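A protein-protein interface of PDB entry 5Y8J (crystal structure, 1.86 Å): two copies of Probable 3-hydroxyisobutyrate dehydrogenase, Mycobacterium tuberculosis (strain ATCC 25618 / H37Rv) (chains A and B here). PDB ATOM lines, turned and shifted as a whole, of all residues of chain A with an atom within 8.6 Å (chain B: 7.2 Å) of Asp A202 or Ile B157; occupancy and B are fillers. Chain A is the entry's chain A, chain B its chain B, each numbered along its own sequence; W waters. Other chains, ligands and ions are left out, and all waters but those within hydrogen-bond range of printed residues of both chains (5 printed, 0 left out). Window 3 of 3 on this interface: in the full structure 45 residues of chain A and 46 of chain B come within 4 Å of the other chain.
Of the printed residues of chain B, Leu A195 touches Cys B159 (3.2 Å) and Ala B168 (3.6 Å).
Printed residues of chain B within 4 Å of Asp A202: Ile B157 (3.99 Å).
Of the printed residues of chain B, Val A203 touches Met B134, Ile B157, Cys B159 and Ala B168.
Ile A204 touches none of the printed residues of chain B.
Printed residues of chain B within 4 Å of Gly A206: Lys B155.
Of the printed residues of chain A, Met B134 touches Val A203.
Printed residues of chain A within 4 Å of Ile B157: Asp A202 and Val A203.
Printed residues of chain A within 4 Å of Ala B168: Leu A195 (3.6 Å) and Val A203 (3.8 Å).
The nearest printed residue of chain B that does not touch Asp A202 is Lys B155 (5.9 Å).
The nearest printed residue of chain A that does not touch Ile B157 is Ser A199 (5.1 Å).
The backbone carbonyl oxygen (O) of Val B135 is in hydrogen-bond range of the backbone NH (N) of Cys B159 (2.7 Å).
SG of Cys B159 sits at hydrogen-bond distance from O of Ile B157.
N of Val B135 lies within hydrogen-bond range of O of Ile B157 (2.9 Å).
OG of Ser A196 is in hydrogen-bond range of OG of Ser A199.
The backbone carbonyl oxygen (O) of Lys B155 is in hydrogen-bond range of the backbone NH (N) of Phe B133, 2.8 Å away.
The backbone carbonyl oxygen of Phe B133 lies within hydrogen-bond range of the backbone NH of Ile B157, 2.8 Å away.
Water W5 lies within hydrogen-bond range of OG of Ser A199 (2.5 Å) and O of His B158 (2.6 Å).
Water W4 lies within hydrogen-bond range of NZ of Lys B155 (2.7 Å) and O of Asp A202 (3.4 Å).
Water W3 lies within hydrogen-bond range of O of Cys B159 (2.8 Å), N of Ser A196 (2.9 Å) and OG of Ser A199 (3.3 Å).
Water W1 bridges O of Gly A206 (2.9 Å) and NZ of Lys B155 (3.3 Å).
Water W2 lies within hydrogen-bond range of the backbone carbonyl oxygen of His B158 (3.2 Å) and the backbone carbonyl oxygen of Ser A199 (3.2 Å).
No position is printed for both chains.
Printed residues of chain A that touch a printed residue of chain B: Leu A195, Ser A199, Asp A202, Val A203 and Gly A206.
Of the 16 printed residues of chain B, 5 touch a printed residue of chain A.
Hydrophobic or aromatic side chains of chain B that line the printed part of chain A: Met B134, Ile B157 and Ala B168.
Among the printed residues, 9 pairs touch across the chains.
The backbone carbonyl oxygen (O) of Cys B159 is in hydrogen-bond range of the side-chain hydroxyl (OG) of Ser A199 (3.1 Å).
O of Gly A206 lies within hydrogen-bond range of NZ of Lys B155 (3.0 Å).
CD1 of Leu A195 touches O of Cys B159 (3.2 Å).
Leu A195 touches Ala B168 (CD2 to CA, 3.6 Å).
Ile B157 touches Asp A202.
Val A203 touches Met B134 (CG1 to SD, 3.97 Å).
Val A203 touches Ile B157.
Cys B159 touches Val A203 (SG to CG2, 3.7 Å).
Ala B168 touches Val A203 (CB to CG2, 3.8 Å).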
ATOM      1  N   PHE A 187     -10.481   7.114  25.119  1.00  0.00           N
ATOM      2  CA  PHE A 187     -10.636   6.709  23.721  1.00  0.00           C
ATOM      3  C   PHE A 187     -10.585   7.885  22.744  1.00  0.00           C
ATOM      4  O   PHE A 187      -9.987   7.756  21.680  1.00  0.00           O
ATOM      5  CB  PHE A 187     -11.899   5.853  23.456  1.00  0.00           C
ATOM      6  CG  PHE A 187     -11.681   4.438  23.782  1.00  0.00           C
ATOM      7  CD1 PHE A 187     -11.044   3.603  22.882  1.00  0.00           C
ATOM      8  CD2 PHE A 187     -11.959   3.950  25.080  1.00  0.00           C
ATOM      9  CE1 PHE A 187     -10.757   2.297  23.215  1.00  0.00           C
ATOM     10  CE2 PHE A 187     -11.715   2.634  25.386  1.00  0.00           C
ATOM     11  CZ  PHE A 187     -11.082   1.800  24.448  1.00  0.00           C
ATOM     12  N   LEU A 195      -3.545   6.809  18.110  1.00  0.00           N
ATOM     13  CA  LEU A 195      -3.513   5.476  18.698  1.00  0.00           C
ATOM     14  C   LEU A 195      -4.847   4.831  18.425  1.00  0.00           C
ATOM     15  O   LEU A 195      -5.927   5.408  18.825  1.00  0.00           O
ATOM     16  CB  LEU A 195      -3.285   5.609  20.208  1.00  0.00           C
ATOM     17  CG  LEU A 195      -3.326   4.408  21.099  1.00  0.00           C
ATOM     18  CD1 LEU A 195      -2.192   3.440  20.763  1.00  0.00           C
ATOM     19  CD2 LEU A 195      -3.214   4.916  22.528  1.00  0.00           C
ATOM     20  N   SER A 196      -4.816   3.664  17.762  1.00  0.00           N
ATOM     21  CA  SER A 196      -6.064   2.991  17.378  1.00  0.00           C
ATOM     22  C   SER A 196      -6.901   2.598  18.659  1.00  0.00           C
ATOM     23  O   SER A 196      -6.356   2.345  19.754  1.00  0.00           O
ATOM     24  CB  SER A 196      -5.833   1.752  16.508  1.00  0.00           C
ATOM     25  OG  SER A 196      -5.363   0.667  17.293  1.00  0.00           O
ATOM     26  N   ALA A 197      -8.211   2.459  18.470  1.00  0.00           N
ATOM     27  CA  ALA A 197      -9.105   2.005  19.517  1.00  0.00           C
ATOM     28  C   ALA A 197      -8.761   0.636  19.988  1.00  0.00           C
ATOM     29  O   ALA A 197      -8.763   0.366  21.192  1.00  0.00           O
ATOM     30  CB  ALA A 197     -10.584   2.001  18.986  1.00  0.00           C
ATOM     31  N   GLN A 198      -8.465  -0.279  19.080  1.00  0.00           N
ATOM     32  CA  GLN A 198      -8.106  -1.636  19.480  1.00  0.00           C
ATOM     33  C   GLN A 198      -6.802  -1.655  20.293  1.00  0.00           C
ATOM     34  O   GLN A 198      -6.697  -2.422  21.265  1.00  0.00           O
ATOM     35  CB  GLN A 198      -8.023  -2.615  18.292  1.00  0.00           C
ATOM     36  CG  GLN A 198      -7.793  -4.059  18.697  1.00  0.00           C
ATOM     37  CD  GLN A 198      -9.016  -4.655  19.346  1.00  0.00           C
ATOM     38  OE1 GLN A 198     -10.123  -4.550  18.794  1.00  0.00           O
ATOM     39  NE2 GLN A 198      -8.854  -5.243  20.497  1.00  0.00           N
ATOM     40  N   SER A 199      -5.825  -0.819  19.913  1.00  0.00           N
ATOM     41  CA  SER A 199      -4.551  -0.736  20.637  1.00  0.00           C
ATOM     42  C   SER A 199      -4.748  -0.205  22.053  1.00  0.00           C
ATOM     43  O   SER A 199      -4.203  -0.777  22.995  1.00  0.00           O
ATOM     44  CB  SER A 199      -3.528   0.124  19.905  1.00  0.00           C
ATOM     45  OG  SER A 199      -3.115  -0.485  18.685  1.00  0.00           O
ATOM     46  N   LEU A 200      -5.499   0.888  22.199  1.00  0.00           N
ATOM     47  CA  LEU A 200      -5.829   1.396  23.506  1.00  0.00           C
ATOM     48  C   LEU A 200      -6.588   0.363  24.341  1.00  0.00           C
ATOM     49  O   LEU A 200      -6.278   0.151  25.545  1.00  0.00           O
ATOM     50  CB  LEU A 200      -6.595   2.676  23.486  1.00  0.00           C
ATOM     51  CG  LEU A 200      -6.857   3.248  24.876  1.00  0.00           C
ATOM     52  CD1 LEU A 200      -5.625   3.782  25.594  1.00  0.00           C
ATOM     53  CD2 LEU A 200      -7.982   4.276  24.910  1.00  0.00           C
ATOM     54  N   PHE A 201      -7.595  -0.253  23.738  1.00  0.00           N
ATOM     55  CA  PHE A 201      -8.326  -1.299  24.456  1.00  0.00           C
ATOM     56  C   PHE A 201      -7.407  -2.409  24.984  1.00  0.00           C
ATOM     57  O   PHE A 201      -7.461  -2.776  26.183  1.00  0.00           O
ATOM     58  CB  PHE A 201      -9.399  -1.919  23.561  1.00  0.00           C
ATOM     59  CG  PHE A 201     -10.159  -3.038  24.210  1.00  0.00           C
ATOM     60  CD1 PHE A 201     -11.339  -2.775  24.882  1.00  0.00           C
ATOM     61  CD2 PHE A 201      -9.752  -4.345  24.101  1.00  0.00           C
ATOM     62  CE1 PHE A 201     -12.051  -3.773  25.453  1.00  0.00           C
ATOM     63  CE2 PHE A 201     -10.481  -5.367  24.680  1.00  0.00           C
ATOM     64  CZ  PHE A 201     -11.652  -5.085  25.343  1.00  0.00           C
ATOM     65  N   ASP A 202      -6.551  -2.934  24.129  1.00  0.00           N
ATOM     66  CA  ASP A 202      -5.562  -3.992  24.510  1.00  0.00           C
ATOM     67  C   ASP A 202      -4.697  -3.527  25.659  1.00  0.00           C
ATOM     68  O   ASP A 202      -4.408  -4.287  26.555  1.00  0.00           O
ATOM     69  CB  ASP A 202      -4.698  -4.436  23.309  1.00  0.00           C
ATOM     70  CG  ASP A 202      -5.487  -5.135  22.240  1.00  0.00           C
ATOM     71  OD1 ASP A 202      -6.686  -5.491  22.463  1.00  0.00           O
ATOM     72  OD2 ASP A 202      -4.977  -5.309  21.117  1.00  0.00           O
ATOM     73  N   VAL A 203      -4.259  -2.261  25.648  1.00  0.00           N
ATOM     74  CA  VAL A 203      -3.405  -1.798  26.729  1.00  0.00           C
ATOM     75  C   VAL A 203      -4.154  -1.627  28.025  1.00  0.00           C
ATOM     76  O   VAL A 203      -3.749  -2.209  29.043  1.00  0.00           O
ATOM     77  CB  VAL A 203      -2.668  -0.472  26.424  1.00  0.00           C
ATOM     78  CG1 VAL A 203      -1.833   0.010  27.630  1.00  0.00           C
ATOM     79  CG2 VAL A 203      -1.693  -0.683  25.285  1.00  0.00           C
ATOM     80  N   ILE A 204      -5.198  -0.815  28.016  1.00  0.00           N
ATOM     81  CA  ILE A 204      -5.955  -0.526  29.235  1.00  0.00           C
ATOM     82  C   ILE A 204      -6.486  -1.776  29.915  1.00  0.00           C
ATOM     83  O   ILE A 204      -6.411  -1.915  31.084  1.00  0.00           O
ATOM     84  CB  ILE A 204      -7.131   0.418  28.998  1.00  0.00           C
ATOM     85  CG1 ILE A 204      -6.648   1.744  28.473  1.00  0.00           C
ATOM     86  CG2 ILE A 204      -7.882   0.589  30.284  1.00  0.00           C
ATOM     87  CD1 ILE A 204      -7.605   2.893  28.670  1.00  0.00           C
ATOM     88  N   THR A 205      -7.003  -2.686  29.130  1.00  0.00           N
ATOM     89  CA  THR A 205      -7.560  -3.938  29.722  1.00  0.00           C
ATOM     90  C   THR A 205      -6.522  -4.837  30.336  1.00  0.00           C
ATOM     91  O   THR A 205      -6.829  -5.615  31.247  1.00  0.00           O
ATOM     92  CB  THR A 205      -8.452  -4.728  28.777  1.00  0.00           C
ATOM     93  OG1 THR A 205      -7.715  -5.163  27.662  1.00  0.00           O
ATOM     94  CG2 THR A 205      -9.666  -3.832  28.299  1.00  0.00           C
ATOM     95  N   GLY A 206      -5.272  -4.695  29.887  1.00  0.00           N
ATOM     96  CA  GLY A 206      -4.127  -5.394  30.483  1.00  0.00           C
ATOM     97  C   GLY A 206      -3.405  -4.573  31.531  1.00  0.00           C
ATOM     98  O   GLY A 206      -2.395  -4.995  32.056  1.00  0.00           O
ATOM     99  N   ALA A 207      -3.883  -3.382  31.851  1.00  0.00           N
ATOM    100  CA  ALA A 207      -3.160  -2.479  32.756  1.00  0.00           C
ATOM    101  C   ALA A 207      -4.037  -1.970  33.895  1.00  0.00           C
ATOM    102  O   ALA A 207      -5.205  -2.435  34.088  1.00  0.00           O
ATOM    103  CB  ALA A 207      -2.588  -1.335  31.917  1.00  0.00           C
ATOM    104  N   ASN A 210      -7.951  -0.788  33.741  1.00  0.00           N
ATOM    105  CA  ASN A 210      -9.058  -1.679  33.351  1.00  0.00           C
ATOM    106  C   ASN A 210     -10.276  -1.577  34.297  1.00  0.00           C
ATOM    107  O   ASN A 210     -10.150  -1.483  35.540  1.00  0.00           O
ATOM    108  CB  ASN A 210      -8.604  -3.138  33.371  1.00  0.00           C
ATOM    109  CG  ASN A 210      -9.574  -4.047  32.637  1.00  0.00           C
ATOM    110  OD1 ASN A 210     -10.324  -3.627  31.794  1.00  0.00           O
ATOM    111  ND2 ASN A 210      -9.548  -5.308  32.981  1.00  0.00           N
ATOM    112  N   VAL A 214     -14.765  -0.265  30.282  1.00  0.00           N
ATOM    113  CA  VAL A 214     -14.081  -0.563  29.057  1.00  0.00           C
ATOM    114  C   VAL A 214     -14.215  -2.031  28.685  1.00  0.00           C
ATOM    115  O   VAL A 214     -14.470  -2.328  27.523  1.00  0.00           O
ATOM    116  CB  VAL A 214     -12.600  -0.037  29.038  1.00  0.00           C
ATOM    117  CG1 VAL A 214     -11.780  -0.504  30.238  1.00  0.00           C
ATOM    118  CG2 VAL A 214     -11.904  -0.410  27.705  1.00  0.00           C
ATOM    119  N   CYS A 218     -17.238  -0.951  26.478  1.00  0.00           N
ATOM    120  CA  CYS A 218     -16.353  -0.179  25.558  1.00  0.00           C
ATOM    121  C   CYS A 218     -17.167   0.802  24.689  1.00  0.00           C
ATOM    122  O   CYS A 218     -18.015   0.339  23.888  1.00  0.00           O
ATOM    123  CB  CYS A 218     -15.633  -1.142  24.642  1.00  0.00           C
ATOM    124  SG  CYS A 218     -14.432  -0.251  23.644  1.00  0.00           S
ATOM    125  N   PRO A 223     -13.950  -3.223  19.616  1.00  0.00           N
ATOM    126  CA  PRO A 223     -13.176  -4.093  20.531  1.00  0.00           C
ATOM    127  C   PRO A 223     -14.024  -5.028  21.384  1.00  0.00           C
ATOM    128  O   PRO A 223     -13.526  -6.080  21.849  1.00  0.00           O
ATOM    129  CB  PRO A 223     -12.454  -3.091  21.415  1.00  0.00           C
ATOM    130  CG  PRO A 223     -12.308  -1.852  20.601  1.00  0.00           C
ATOM    131  CD  PRO A 223     -13.535  -1.817  19.679  1.00  0.00           C
ATOM    132  N   ASP B 116       9.800   4.312  20.807  1.00  0.00           N
ATOM    133  CA  ASP B 116       9.399   4.720  22.151  1.00  0.00           C
ATOM    134  C   ASP B 116       8.919   3.504  22.866  1.00  0.00           C
ATOM    135  O   ASP B 116       8.104   2.731  22.325  1.00  0.00           O
ATOM    136  CB  ASP B 116       8.336   5.831  22.238  1.00  0.00           C
ATOM    137  CG  ASP B 116       7.123   5.600  21.414  1.00  0.00           C
ATOM    138  OD1 ASP B 116       7.286   5.486  20.181  1.00  0.00           O
ATOM    139  OD2 ASP B 116       5.962   5.635  21.941  1.00  0.00           O
ATOM    140  N   ALA B 132       6.064  -3.630  32.198  1.00  0.00           N
ATOM    141  CA  ALA B 132       5.379  -3.642  30.924  1.00  0.00           C
ATOM    142  C   ALA B 132       5.942  -2.566  30.026  1.00  0.00           C
ATOM    143  O   ALA B 132       5.892  -1.395  30.386  1.00  0.00           O
ATOM    144  CB  ALA B 132       3.908  -3.417  31.149  1.00  0.00           C
ATOM    145  N   PHE B 133       6.408  -2.956  28.864  1.00  0.00           N
ATOM    146  CA  PHE B 133       6.886  -2.025  27.800  1.00  0.00           C
ATOM    147  C   PHE B 133       5.744  -1.782  26.825  1.00  0.00           C
ATOM    148  O   PHE B 133       5.233  -2.724  26.202  1.00  0.00           O
ATOM    149  CB  PHE B 133       8.078  -2.570  27.042  1.00  0.00           C
ATOM    150  CG  PHE B 133       9.372  -2.573  27.836  1.00  0.00           C
ATOM    151  CD1 PHE B 133       9.597  -3.524  28.766  1.00  0.00           C
ATOM    152  CD2 PHE B 133      10.343  -1.585  27.667  1.00  0.00           C
ATOM    153  CE1 PHE B 133      10.769  -3.533  29.543  1.00  0.00           C
ATOM    154  CE2 PHE B 133      11.513  -1.576  28.404  1.00  0.00           C
ATOM    155  CZ  PHE B 133      11.725  -2.534  29.358  1.00  0.00           C
ATOM    156  N   MET B 134       5.394  -0.497  26.671  1.00  0.00           N
ATOM    157  CA  MET B 134       4.408  -0.078  25.689  1.00  0.00           C
ATOM    158  C   MET B 134       5.135   0.603  24.567  1.00  0.00           C
ATOM    159  O   MET B 134       5.658   1.678  24.753  1.00  0.00           O
ATOM    160  CB  MET B 134       3.368   0.818  26.359  1.00  0.00           C
ATOM    161  CG  MET B 134       2.499   0.013  27.374  1.00  0.00           C
ATOM    162  SD  MET B 134       1.835   1.123  28.645  1.00  0.00           S
ATOM    163  CE  MET B 134       3.326   1.319  29.673  1.00  0.00           C
ATOM    164  N   VAL B 135       5.171  -0.029  23.409  1.00  0.00           N
ATOM    165  CA  VAL B 135       6.092   0.327  22.308  1.00  0.00           C
ATOM    166  C   VAL B 135       5.399   1.006  21.144  1.00  0.00           C
ATOM    167  O   VAL B 135       4.357   0.528  20.650  1.00  0.00           O
ATOM    168  CB  VAL B 135       6.721  -0.942  21.763  1.00  0.00           C
ATOM    169  CG1 VAL B 135       7.664  -0.610  20.587  1.00  0.00           C
ATOM    170  CG2 VAL B 135       7.540  -1.599  22.891  1.00  0.00           C
ATOM    171  N   GLY B 136       6.009   2.064  20.647  1.00  0.00           N
ATOM    172  CA  GLY B 136       5.634   2.725  19.412  1.00  0.00           C
ATOM    173  C   GLY B 136       6.770   2.643  18.440  1.00  0.00           C
ATOM    174  O   GLY B 136       7.977   2.774  18.835  1.00  0.00           O
ATOM    175  N   LEU B 142      10.765  -3.504  16.374  1.00  0.00           N
ATOM    176  CA  LEU B 142      10.437  -4.160  17.618  1.00  0.00           C
ATOM    177  C   LEU B 142      10.938  -5.616  17.638  1.00  0.00           C
ATOM    178  O   LEU B 142      11.371  -6.127  18.651  1.00  0.00           O
ATOM    179  CB  LEU B 142       8.881  -4.107  17.892  1.00  0.00           C
ATOM    180  CG  LEU B 142       8.384  -4.832  19.118  1.00  0.00           C
ATOM    181  CD1 LEU B 142       9.197  -4.492  20.360  1.00  0.00           C
ATOM    182  CD2 LEU B 142       6.942  -4.632  19.432  1.00  0.00           C
ATOM    183  N   ARG B 146      13.222  -7.081  20.527  1.00  0.00           N
ATOM    184  CA  ARG B 146      12.657  -8.023  21.526  1.00  0.00           C
ATOM    185  C   ARG B 146      13.635  -8.741  22.418  1.00  0.00           C
ATOM    186  O   ARG B 146      13.452  -8.793  23.644  1.00  0.00           O
ATOM    187  CB  ARG B 146      11.763  -9.133  20.883  1.00  0.00           C
ATOM    188  CG  ARG B 146      10.320  -8.854  20.813  1.00  0.00           C
ATOM    189  CD  ARG B 146       9.442 -10.075  20.808  1.00  0.00           C
ATOM    190  NE  ARG B 146       8.228  -9.709  21.584  1.00  0.00           N
ATOM    191  CZ  ARG B 146       7.226  -8.996  21.090  1.00  0.00           C
ATOM    192  NH1 ARG B 146       7.262  -8.585  19.823  1.00  0.00           N
ATOM    193  NH2 ARG B 146       6.171  -8.707  21.848  1.00  0.00           N
ATOM    194  N   LYS B 155       5.868  -7.887  30.198  1.00  0.00           N
ATOM    195  CA  LYS B 155       4.984  -7.745  29.026  1.00  0.00           C
ATOM    196  C   LYS B 155       5.576  -6.729  28.036  1.00  0.00           C
ATOM    197  O   LYS B 155       6.147  -5.668  28.462  1.00  0.00           O
ATOM    198  CB  LYS B 155       3.639  -7.224  29.530  1.00  0.00           C
ATOM    199  CG  LYS B 155       2.623  -7.053  28.472  1.00  0.00           C
ATOM    200  CD  LYS B 155       1.241  -7.415  29.008  1.00  0.00           C
ATOM    201  CE  LYS B 155       0.755  -6.408  30.024  1.00  0.00           C
ATOM    202  NZ  LYS B 155      -0.660  -6.779  30.364  1.00  0.00           N
ATOM    203  N   ILE B 156       5.520  -7.073  26.741  1.00  0.00           N
ATOM    204  CA  ILE B 156       5.884  -6.156  25.631  1.00  0.00           C
ATOM    205  C   ILE B 156       4.628  -6.018  24.770  1.00  0.00           C
ATOM    206  O   ILE B 156       4.124  -7.008  24.264  1.00  0.00           O
ATOM    207  CB  ILE B 156       7.048  -6.722  24.837  1.00  0.00           C
ATOM    208  CG1 ILE B 156       8.255  -6.885  25.749  1.00  0.00           C
ATOM    209  CG2 ILE B 156       7.390  -5.928  23.585  1.00  0.00           C
ATOM    210  CD1 ILE B 156       9.343  -7.795  25.146  1.00  0.00           C
ATOM    211  N   ILE B 157       4.117  -4.792  24.609  1.00  0.00           N
ATOM    212  CA  ILE B 157       2.959  -4.590  23.773  1.00  0.00           C
ATOM    213  C   ILE B 157       3.211  -3.532  22.741  1.00  0.00           C
ATOM    214  O   ILE B 157       3.611  -2.420  23.053  1.00  0.00           O
ATOM    215  CB  ILE B 157       1.675  -4.436  24.615  1.00  0.00           C
ATOM    216  CG1 ILE B 157       0.470  -4.075  23.718  1.00  0.00           C
ATOM    217  CG2 ILE B 157       1.821  -3.426  25.685  1.00  0.00           C
ATOM    218  CD1 ILE B 157      -0.863  -4.322  24.419  1.00  0.00           C
ATOM    219  N   HIS B 158       3.015  -3.907  21.506  1.00  0.00           N
ATOM    220  CA  HIS B 158       3.147  -2.988  20.393  1.00  0.00           C
ATOM    221  C   HIS B 158       1.911  -2.140  20.220  1.00  0.00           C
ATOM    222  O   HIS B 158       0.827  -2.680  19.956  1.00  0.00           O
ATOM    223  CB  HIS B 158       3.441  -3.735  19.083  1.00  0.00           C
ATOM    224  CG  HIS B 158       3.866  -2.797  18.004  1.00  0.00           C
ATOM    225  ND1 HIS B 158       3.825  -3.109  16.678  1.00  0.00           N
ATOM    226  CD2 HIS B 158       4.448  -1.576  18.070  1.00  0.00           C
ATOM    227  CE1 HIS B 158       4.269  -2.085  15.973  1.00  0.00           C
ATOM    228  NE2 HIS B 158       4.665  -1.152  16.795  1.00  0.00           N
ATOM    229  N   CYS B 159       2.034  -0.831  20.361  1.00  0.00           N
ATOM    230  CA  CYS B 159       0.887   0.046  20.460  1.00  0.00           C
ATOM    231  C   CYS B 159       0.555   0.772  19.153  1.00  0.00           C
ATOM    232  O   CYS B 159      -0.570   1.257  19.031  1.00  0.00           O
ATOM    233  CB  CYS B 159       1.141   1.086  21.561  1.00  0.00           C
ATOM    234  SG  CYS B 159       1.230   0.335  23.194  1.00  0.00           S
ATOM    235  N   GLY B 160       1.477   0.778  18.172  1.00  0.00           N
ATOM    236  CA  GLY B 160       1.274   1.467  16.937  1.00  0.00           C
ATOM    237  C   GLY B 160       2.593   2.161  16.510  1.00  0.00           C
ATOM    238  O   GLY B 160       3.687   1.752  16.930  1.00  0.00           O
ATOM    239  N   GLY B 165       3.420   4.271  22.097  1.00  0.00           N
ATOM    240  CA  GLY B 165       3.696   3.805  23.410  1.00  0.00           C
ATOM    241  C   GLY B 165       3.435   4.850  24.430  1.00  0.00           C
ATOM    242  O   GLY B 165       2.776   4.594  25.466  1.00  0.00           O
ATOM    243  N   ALA B 168      -0.356   5.404  24.698  1.00  0.00           N
ATOM    244  CA  ALA B 168      -1.106   4.386  25.392  1.00  0.00           C
ATOM    245  C   ALA B 168      -0.866   4.521  26.904  1.00  0.00           C
ATOM    246  O   ALA B 168      -1.811   4.486  27.689  1.00  0.00           O
ATOM    247  CB  ALA B 168      -0.729   3.020  24.897  1.00  0.00           C
HETATM  248  O   HOH W   1       0.160  -3.758  31.517  1.00  0.00           O
HETATM  249  O   HOH W   2      -1.728  -2.303  21.763  1.00  0.00           O
HETATM  250  O   HOH W   3      -2.340   2.324  17.142  1.00  0.00           O
HETATM  251  O   HOH W   4      -1.713  -5.882  27.998  1.00  0.00           O
HETATM  252  O   HOH W   5      -1.379  -2.258  18.561  1.00  0.00           O
